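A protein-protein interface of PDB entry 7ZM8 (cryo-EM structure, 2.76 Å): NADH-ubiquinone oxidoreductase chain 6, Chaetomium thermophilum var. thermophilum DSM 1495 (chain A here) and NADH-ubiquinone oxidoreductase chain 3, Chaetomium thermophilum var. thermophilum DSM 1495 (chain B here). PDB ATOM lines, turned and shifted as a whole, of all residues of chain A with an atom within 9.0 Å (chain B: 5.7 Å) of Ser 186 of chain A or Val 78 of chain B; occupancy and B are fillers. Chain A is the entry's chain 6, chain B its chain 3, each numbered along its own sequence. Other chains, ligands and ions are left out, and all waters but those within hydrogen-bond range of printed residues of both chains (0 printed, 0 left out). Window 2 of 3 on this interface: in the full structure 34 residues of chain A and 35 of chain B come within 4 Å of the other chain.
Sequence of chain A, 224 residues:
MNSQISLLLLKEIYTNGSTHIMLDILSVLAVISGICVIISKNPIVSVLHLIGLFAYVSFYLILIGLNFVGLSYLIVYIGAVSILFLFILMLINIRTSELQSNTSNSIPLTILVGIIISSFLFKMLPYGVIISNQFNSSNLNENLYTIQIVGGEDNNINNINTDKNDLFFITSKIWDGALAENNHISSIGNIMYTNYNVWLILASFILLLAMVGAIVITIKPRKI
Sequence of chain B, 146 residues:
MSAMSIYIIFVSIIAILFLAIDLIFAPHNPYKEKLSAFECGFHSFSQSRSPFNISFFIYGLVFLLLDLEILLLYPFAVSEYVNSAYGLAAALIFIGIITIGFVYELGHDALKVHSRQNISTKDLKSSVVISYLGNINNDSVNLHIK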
ATOM      1  N   PHE A  68       6.573  32.823  -7.356  1.00  0.00           N
ATOM      2  CA  PHE A  68       6.483  32.314  -8.747  1.00  0.00           C
ATOM      3  C   PHE A  68       6.975  33.380  -9.721  1.00  0.00           C
ATOM      4  O   PHE A  68       7.731  33.024 -10.618  1.00  0.00           O
ATOM      5  CB  PHE A  68       5.020  32.015  -9.091  1.00  0.00           C
ATOM      6  CG  PHE A  68       4.716  31.807 -10.551  1.00  0.00           C
ATOM      7  CD1 PHE A  68       5.263  30.742 -11.247  1.00  0.00           C
ATOM      8  CD2 PHE A  68       3.858  32.661 -11.222  1.00  0.00           C
ATOM      9  CE1 PHE A  68       4.974  30.551 -12.589  1.00  0.00           C
ATOM     10  CE2 PHE A  68       3.570  32.468 -12.563  1.00  0.00           C
ATOM     11  CZ  PHE A  68       4.128  31.414 -13.243  1.00  0.00           C
ATOM     12  N   ALA A 180      -9.007  26.715   2.001  1.00  0.00           N
ATOM     13  CA  ALA A 180      -8.228  26.060   0.943  1.00  0.00           C
ATOM     14  C   ALA A 180      -7.317  27.100   0.316  1.00  0.00           C
ATOM     15  O   ALA A 180      -7.499  27.387  -0.856  1.00  0.00           O
ATOM     16  CB  ALA A 180      -9.197  25.536  -0.068  1.00  0.00           C
ATOM     17  N   GLU A 181      -6.348  27.614   1.051  1.00  0.00           N
ATOM     18  CA  GLU A 181      -5.512  28.707   0.507  1.00  0.00           C
ATOM     19  C   GLU A 181      -4.709  28.207  -0.692  1.00  0.00           C
ATOM     20  O   GLU A 181      -4.213  27.066  -0.663  1.00  0.00           O
ATOM     21  CB  GLU A 181      -4.670  29.380   1.593  1.00  0.00           C
ATOM     22  CG  GLU A 181      -3.516  30.226   1.089  1.00  0.00           C
ATOM     23  CD  GLU A 181      -2.164  29.530   1.118  1.00  0.00           C
ATOM     24  OE1 GLU A 181      -2.082  28.431   1.697  1.00  0.00           O
ATOM     25  OE2 GLU A 181      -1.200  30.084   0.556  1.00  0.00           O
ATOM     26  N   ASN A 182      -4.570  29.060  -1.702  1.00  0.00           N
ATOM     27  CA  ASN A 182      -3.862  28.654  -2.929  1.00  0.00           C
ATOM     28  C   ASN A 182      -2.535  29.376  -2.986  1.00  0.00           C
ATOM     29  O   ASN A 182      -2.428  30.442  -2.374  1.00  0.00           O
ATOM     30  CB  ASN A 182      -4.628  29.000  -4.207  1.00  0.00           C
ATOM     31  CG  ASN A 182      -5.985  28.350  -4.324  1.00  0.00           C
ATOM     32  OD1 ASN A 182      -6.373  27.538  -3.493  1.00  0.00           O
ATOM     33  ND2 ASN A 182      -6.715  28.712  -5.360  1.00  0.00           N
ATOM     34  N   ASN A 183      -1.548  28.757  -3.623  1.00  0.00           N
ATOM     35  CA  ASN A 183      -0.282  29.469  -3.886  1.00  0.00           C
ATOM     36  C   ASN A 183      -0.612  30.489  -4.969  1.00  0.00           C
ATOM     37  O   ASN A 183      -1.593  30.281  -5.671  1.00  0.00           O
ATOM     38  CB  ASN A 183       0.783  28.493  -4.359  1.00  0.00           C
ATOM     39  CG  ASN A 183       1.070  27.396  -3.360  1.00  0.00           C
ATOM     40  OD1 ASN A 183       1.089  27.638  -2.155  1.00  0.00           O
ATOM     41  ND2 ASN A 183       1.305  26.191  -3.851  1.00  0.00           N
ATOM     42  N   HIS A 184       0.188  31.526  -5.132  1.00  0.00           N
ATOM     43  CA  HIS A 184      -0.147  32.582  -6.119  1.00  0.00           C
ATOM     44  C   HIS A 184      -0.297  32.007  -7.526  1.00  0.00           C
ATOM     45  O   HIS A 184      -1.171  32.493  -8.226  1.00  0.00           O
ATOM     46  CB  HIS A 184       0.889  33.704  -6.138  1.00  0.00           C
ATOM     47  CG  HIS A 184       1.054  34.439  -4.852  1.00  0.00           C
ATOM     48  ND1 HIS A 184       2.223  35.089  -4.522  1.00  0.00           N
ATOM     49  CD2 HIS A 184       0.211  34.645  -3.824  1.00  0.00           C
ATOM     50  CE1 HIS A 184       2.091  35.661  -3.348  1.00  0.00           C
ATOM     51  NE2 HIS A 184       0.870  35.402  -2.899  1.00  0.00           N
ATOM     52  N   ILE A 185       0.524  31.037  -7.923  1.00  0.00           N
ATOM     53  CA  ILE A 185       0.481  30.436  -9.283  1.00  0.00           C
ATOM     54  C   ILE A 185      -0.880  29.759  -9.482  1.00  0.00           C
ATOM     55  O   ILE A 185      -1.423  29.839 -10.580  1.00  0.00           O
ATOM     56  CB  ILE A 185       1.685  29.485  -9.459  1.00  0.00           C
ATOM     57  CG1 ILE A 185       1.724  28.870 -10.860  1.00  0.00           C
ATOM     58  CG2 ILE A 185       1.742  28.435  -8.363  1.00  0.00           C
ATOM     59  CD1 ILE A 185       2.853  27.906 -11.086  1.00  0.00           C
ATOM     60  N   SER A 186      -1.381  29.067  -8.465  1.00  0.00           N
ATOM     61  CA  SER A 186      -2.707  28.422  -8.521  1.00  0.00           C
ATOM     62  C   SER A 186      -3.794  29.486  -8.643  1.00  0.00           C
ATOM     63  O   SER A 186      -4.706  29.277  -9.419  1.00  0.00           O
ATOM     64  CB  SER A 186      -2.840  27.579  -7.318  1.00  0.00           C
ATOM     65  OG  SER A 186      -1.713  26.732  -7.189  1.00  0.00           O
ATOM     66  N   SER A 187      -3.671  30.586  -7.912  1.00  0.00           N
ATOM     67  CA  SER A 187      -4.603  31.729  -8.030  1.00  0.00           C
ATOM     68  C   SER A 187      -4.520  32.402  -9.412  1.00  0.00           C
ATOM     69  O   SER A 187      -5.580  32.758  -9.937  1.00  0.00           O
ATOM     70  CB  SER A 187      -4.327  32.675  -6.909  1.00  0.00           C
ATOM     71  OG  SER A 187      -4.085  31.968  -5.710  1.00  0.00           O
ATOM     72  N   ILE A 188      -3.321  32.597  -9.960  1.00  0.00           N
ATOM     73  CA  ILE A 188      -3.138  33.175 -11.322  1.00  0.00           C
ATOM     74  C   ILE A 188      -3.748  32.193 -12.301  1.00  0.00           C
ATOM     75  O   ILE A 188      -4.480  32.628 -13.165  1.00  0.00           O
ATOM     76  CB  ILE A 188      -1.645  33.434 -11.620  1.00  0.00           C
ATOM     77  CG1 ILE A 188      -1.087  34.565 -10.754  1.00  0.00           C
ATOM     78  CG2 ILE A 188      -1.426  33.714 -13.098  1.00  0.00           C
ATOM     79  CD1 ILE A 188       0.406  34.736 -10.849  1.00  0.00           C
ATOM     80  N   GLY A 189      -3.515  30.904 -12.086  1.00  0.00           N
ATOM     81  CA  GLY A 189      -4.050  29.842 -12.944  1.00  0.00           C
ATOM     82  C   GLY A 189      -5.553  29.802 -12.920  1.00  0.00           C
ATOM     83  O   GLY A 189      -6.113  29.705 -14.003  1.00  0.00           O
ATOM     84  N   ASN A 190      -6.176  30.013 -11.763  1.00  0.00           N
ATOM     85  CA  ASN A 190      -7.647  29.979 -11.623  1.00  0.00           C
ATOM     86  C   ASN A 190      -8.278  31.010 -12.555  1.00  0.00           C
ATOM     87  O   ASN A 190      -9.375  30.742 -13.036  1.00  0.00           O
ATOM     88  CB  ASN A 190      -8.102  30.239 -10.190  1.00  0.00           C
ATOM     89  CG  ASN A 190      -7.788  29.140  -9.201  1.00  0.00           C
ATOM     90  OD1 ASN A 190      -7.384  28.045  -9.575  1.00  0.00           O
ATOM     91  ND2 ASN A 190      -7.972  29.432  -7.927  1.00  0.00           N
ATOM     92  N   ILE A 191      -7.625  32.136 -12.819  1.00  0.00           N
ATOM     93  CA  ILE A 191      -8.285  33.210 -13.622  1.00  0.00           C
ATOM     94  C   ILE A 191      -7.607  33.404 -14.982  1.00  0.00           C
ATOM     95  O   ILE A 191      -8.249  34.000 -15.858  1.00  0.00           O
ATOM     96  CB  ILE A 191      -8.315  34.513 -12.786  1.00  0.00           C
ATOM     97  CG1 ILE A 191      -6.909  35.060 -12.539  1.00  0.00           C
ATOM     98  CG2 ILE A 191      -9.075  34.312 -11.490  1.00  0.00           C
ATOM     99  CD1 ILE A 191      -6.847  36.556 -12.410  1.00  0.00           C
ATOM    100  N   MET A 192      -6.390  32.889 -15.173  1.00  0.00           N
ATOM    101  CA  MET A 192      -5.594  33.168 -16.362  1.00  0.00           C
ATOM    102  C   MET A 192      -6.192  32.542 -17.615  1.00  0.00           C
ATOM    103  O   MET A 192      -5.990  33.054 -18.722  1.00  0.00           O
ATOM    104  CB  MET A 192      -4.174  32.663 -16.125  1.00  0.00           C
ATOM    105  CG  MET A 192      -3.265  32.614 -17.313  1.00  0.00           C
ATOM    106  SD  MET A 192      -1.614  32.145 -16.794  1.00  0.00           S
ATOM    107  CE  MET A 192      -0.781  32.229 -18.364  1.00  0.00           C
ATOM    108  N   TYR A 193      -6.890  31.413 -17.472  1.00  0.00           N
ATOM    109  CA  TYR A 193      -7.361  30.672 -18.660  1.00  0.00           C
ATOM    110  C   TYR A 193      -8.872  30.741 -18.823  1.00  0.00           C
ATOM    111  O   TYR A 193      -9.390  30.117 -19.736  1.00  0.00           O
ATOM    112  CB  TYR A 193      -6.885  29.223 -18.592  1.00  0.00           C
ATOM    113  CG  TYR A 193      -5.428  29.039 -18.292  1.00  0.00           C
ATOM    114  CD1 TYR A 193      -4.491  29.018 -19.306  1.00  0.00           C
ATOM    115  CD2 TYR A 193      -4.997  28.883 -16.991  1.00  0.00           C
ATOM    116  CE1 TYR A 193      -3.147  28.853 -19.031  1.00  0.00           C
ATOM    117  CE2 TYR A 193      -3.659  28.731 -16.695  1.00  0.00           C
ATOM    118  CZ  TYR A 193      -2.736  28.706 -17.720  1.00  0.00           C
ATOM    119  OH  TYR A 193      -1.426  28.524 -17.423  1.00  0.00           O
ATOM    120  N   TYR B  74       2.481  26.406 -17.034  1.00  0.00           N
ATOM    121  CA  TYR B  74       2.663  25.896 -15.679  1.00  0.00           C
ATOM    122  C   TYR B  74       1.548  26.291 -14.716  1.00  0.00           C
ATOM    123  O   TYR B  74       1.198  25.459 -13.861  1.00  0.00           O
ATOM    124  CB  TYR B  74       4.030  26.330 -15.137  1.00  0.00           C
ATOM    125  CG  TYR B  74       5.111  25.311 -15.394  1.00  0.00           C
ATOM    126  CD1 TYR B  74       5.813  25.307 -16.587  1.00  0.00           C
ATOM    127  CD2 TYR B  74       5.411  24.335 -14.458  1.00  0.00           C
ATOM    128  CE1 TYR B  74       6.789  24.377 -16.836  1.00  0.00           C
ATOM    129  CE2 TYR B  74       6.389  23.394 -14.700  1.00  0.00           C
ATOM    130  CZ  TYR B  74       7.075  23.422 -15.894  1.00  0.00           C
ATOM    131  OH  TYR B  74       8.055  22.498 -16.152  1.00  0.00           O
ATOM    132  N   PRO B  75       0.992  27.508 -14.748  1.00  0.00           N
ATOM    133  CA  PRO B  75      -0.162  27.784 -13.881  1.00  0.00           C
ATOM    134  C   PRO B  75      -1.356  26.890 -14.147  1.00  0.00           C
ATOM    135  O   PRO B  75      -2.111  26.598 -13.215  1.00  0.00           O
ATOM    136  CB  PRO B  75      -0.472  29.255 -14.182  1.00  0.00           C
ATOM    137  CG  PRO B  75       0.790  29.808 -14.658  1.00  0.00           C
ATOM    138  CD  PRO B  75       1.437  28.729 -15.440  1.00  0.00           C
ATOM    139  N   PHE B  76      -1.556  26.449 -15.388  1.00  0.00           N
ATOM    140  CA  PHE B  76      -2.682  25.573 -15.687  1.00  0.00           C
ATOM    141  C   PHE B  76      -2.545  24.235 -14.982  1.00  0.00           C
ATOM    142  O   PHE B  76      -3.535  23.679 -14.499  1.00  0.00           O
ATOM    143  CB  PHE B  76      -2.805  25.366 -17.196  1.00  0.00           C
ATOM    144  CG  PHE B  76      -3.900  24.423 -17.584  1.00  0.00           C
ATOM    145  CD1 PHE B  76      -5.206  24.855 -17.648  1.00  0.00           C
ATOM    146  CD2 PHE B  76      -3.621  23.099 -17.869  1.00  0.00           C
ATOM    147  CE1 PHE B  76      -6.210  23.987 -17.988  1.00  0.00           C
ATOM    148  CE2 PHE B  76      -4.625  22.230 -18.211  1.00  0.00           C
ATOM    149  CZ  PHE B  76      -5.921  22.674 -18.273  1.00  0.00           C
ATOM    150  N   ALA B  77      -1.327  23.696 -14.924  1.00  0.00           N
ATOM    151  CA  ALA B  77      -1.112  22.383 -14.335  1.00  0.00           C
ATOM    152  C   ALA B  77      -1.383  22.358 -12.839  1.00  0.00           C
ATOM    153  O   ALA B  77      -1.805  21.323 -12.319  1.00  0.00           O
ATOM    154  CB  ALA B  77       0.311  21.914 -14.613  1.00  0.00           C
ATOM    155  N   VAL B  78      -1.156  23.465 -12.135  1.00  0.00           N
ATOM    156  CA  VAL B  78      -1.433  23.537 -10.709  1.00  0.00           C
ATOM    157  C   VAL B  78      -2.771  24.206 -10.426  1.00  0.00           C
ATOM    158  O   VAL B  78      -3.017  24.640  -9.300  1.00  0.00           O
ATOM    159  CB  VAL B  78      -0.292  24.239  -9.951  1.00  0.00           C
ATOM    160  CG1 VAL B  78       0.964  23.408 -10.007  1.00  0.00           C
ATOM    161  CG2 VAL B  78      -0.026  25.611 -10.530  1.00  0.00           C
ATOM    162  N   SER B  79      -3.634  24.328 -11.432  1.00  0.00           N
ATOM    163  CA  SER B  79      -4.993  24.802 -11.217  1.00  0.00           C
ATOM    164  C   SER B  79      -5.988  24.058 -12.098  1.00  0.00           C
ATOM    165  O   SER B  79      -7.018  24.618 -12.484  1.00  0.00           O
ATOM    166  CB  SER B  79      -5.090  26.310 -11.450  1.00  0.00           C
ATOM    167  OG  SER B  79      -4.848  26.647 -12.800  1.00  0.00           O
ATOM    168  N   GLU B  80      -5.764  22.784 -12.394  1.00  0.00           N
ATOM    169  CA  GLU B  80      -6.643  22.010 -13.329  1.00  0.00           C
ATOM    170  C   GLU B  80      -8.007  21.658 -12.737  1.00  0.00           C
ATOM    171  O   GLU B  80      -8.946  21.536 -13.511  1.00  0.00           O
ATOM    172  CB  GLU B  80      -5.978  20.714 -13.788  1.00  0.00           C
ATOM    173  CG  GLU B  80      -5.033  20.879 -14.954  1.00  0.00           C
ATOM    174  CD  GLU B  80      -4.055  19.726 -15.070  1.00  0.00           C
ATOM    175  OE1 GLU B  80      -3.606  19.436 -16.194  1.00  0.00           O
ATOM    176  OE2 GLU B  80      -3.750  19.123 -14.032  1.00  0.00           O
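The side-chain hydroxyl of Tyr 193 of chain A is in hydrogen-bond range of the backbone NH of Phe 76 of chain B. The side-chain hydroxyl (OG) of Ser 186 of chain A is in hydrogen-bond range of the backbone carbonyl oxygen (O) of Val 78 of chain B (3.2 Å).
Asn 183 of chain A touches none of the printed residues of chain B. Ser 187 of chain A touches none of the printed residues of chain B. Printed residues of chain B within 4 Å of Met 192 of chain A: Pro 75. Of the printed residues of chain B, Tyr 193 of chain A touches Pro 75 and Phe 76. Of the printed residues of chain A, Phe 76 of chain B touches Tyr 193. No residue of chain A comes within 4 Å of Ala 77 of chain B. Of chain A, only Ile 185 (3.7 Å) and Ser 186 (3.2 Å) come within 4 Å of Val 78 of chain B. The nearest residue of chain B that does not touch Ser 186 of chain A is Pro 75 of chain B (5.1 Å).
Pro 75 of chain B touches Phe 68 of chain A (CG to CZ, 3.97 Å). Ile 185 of chain A touches Pro 75 of chain B. CG1 of Ile 185 of chain A touches CG2 of Val 78 of chain B, 3.7 Å away. Ser 186 of chain A touches Ser 79 of chain B (O to CB, 3.6 Å). O of Pro 75 of chain B touches CA of Gly 189 of chain A, 3.8 Å away. Ser 79 of chain B touches Gly 189 of chain A. Ser 79 of chain B touches Asn 190 of chain A. CG of Pro 75 of chain B touches SD of Met 192 of chain A (3.98 Å). Pro 75 of chain B touches Tyr 193 of chain A.
O of Pro 75 of chain B is in hydrogen-bond range of OG of Ser 79 of chain B (2.8 Å). The side-chain amide nitrogen (ND2) of Asn 182 of chain A lies close to the side-chain amide nitrogen (ND2) of Asn 190 of chain A. The backbone carbonyl oxygen (O) of Ser 186 of chain A lies close to the side-chain amide oxygen (OD1) of Asn 190 of chain A, 3.0 Å away. SD of Met 192 of chain A lies within hydrogen-bond range of OH of Tyr 193 of chain A (3.7 Å).
Printed residues of chain B that touch a printed residue of chain A: Pro 75, Phe 76, Val 78 and Ser 79. Hydrophobic or aromatic side chains of chain B that line the printed part of chain A: Pro 75, Phe 76 and Val 78. Along chain B the printed residues that touch a printed residue of chain A span positions 75 to 79. Of the 15 printed residues of chain A, 7 touch a printed residue of chain B. Hydrophobic or aromatic side chains of chain A within 4 Å of the printed part of chain B: Phe 68, Ile 185, Met 192 and Tyr 193.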
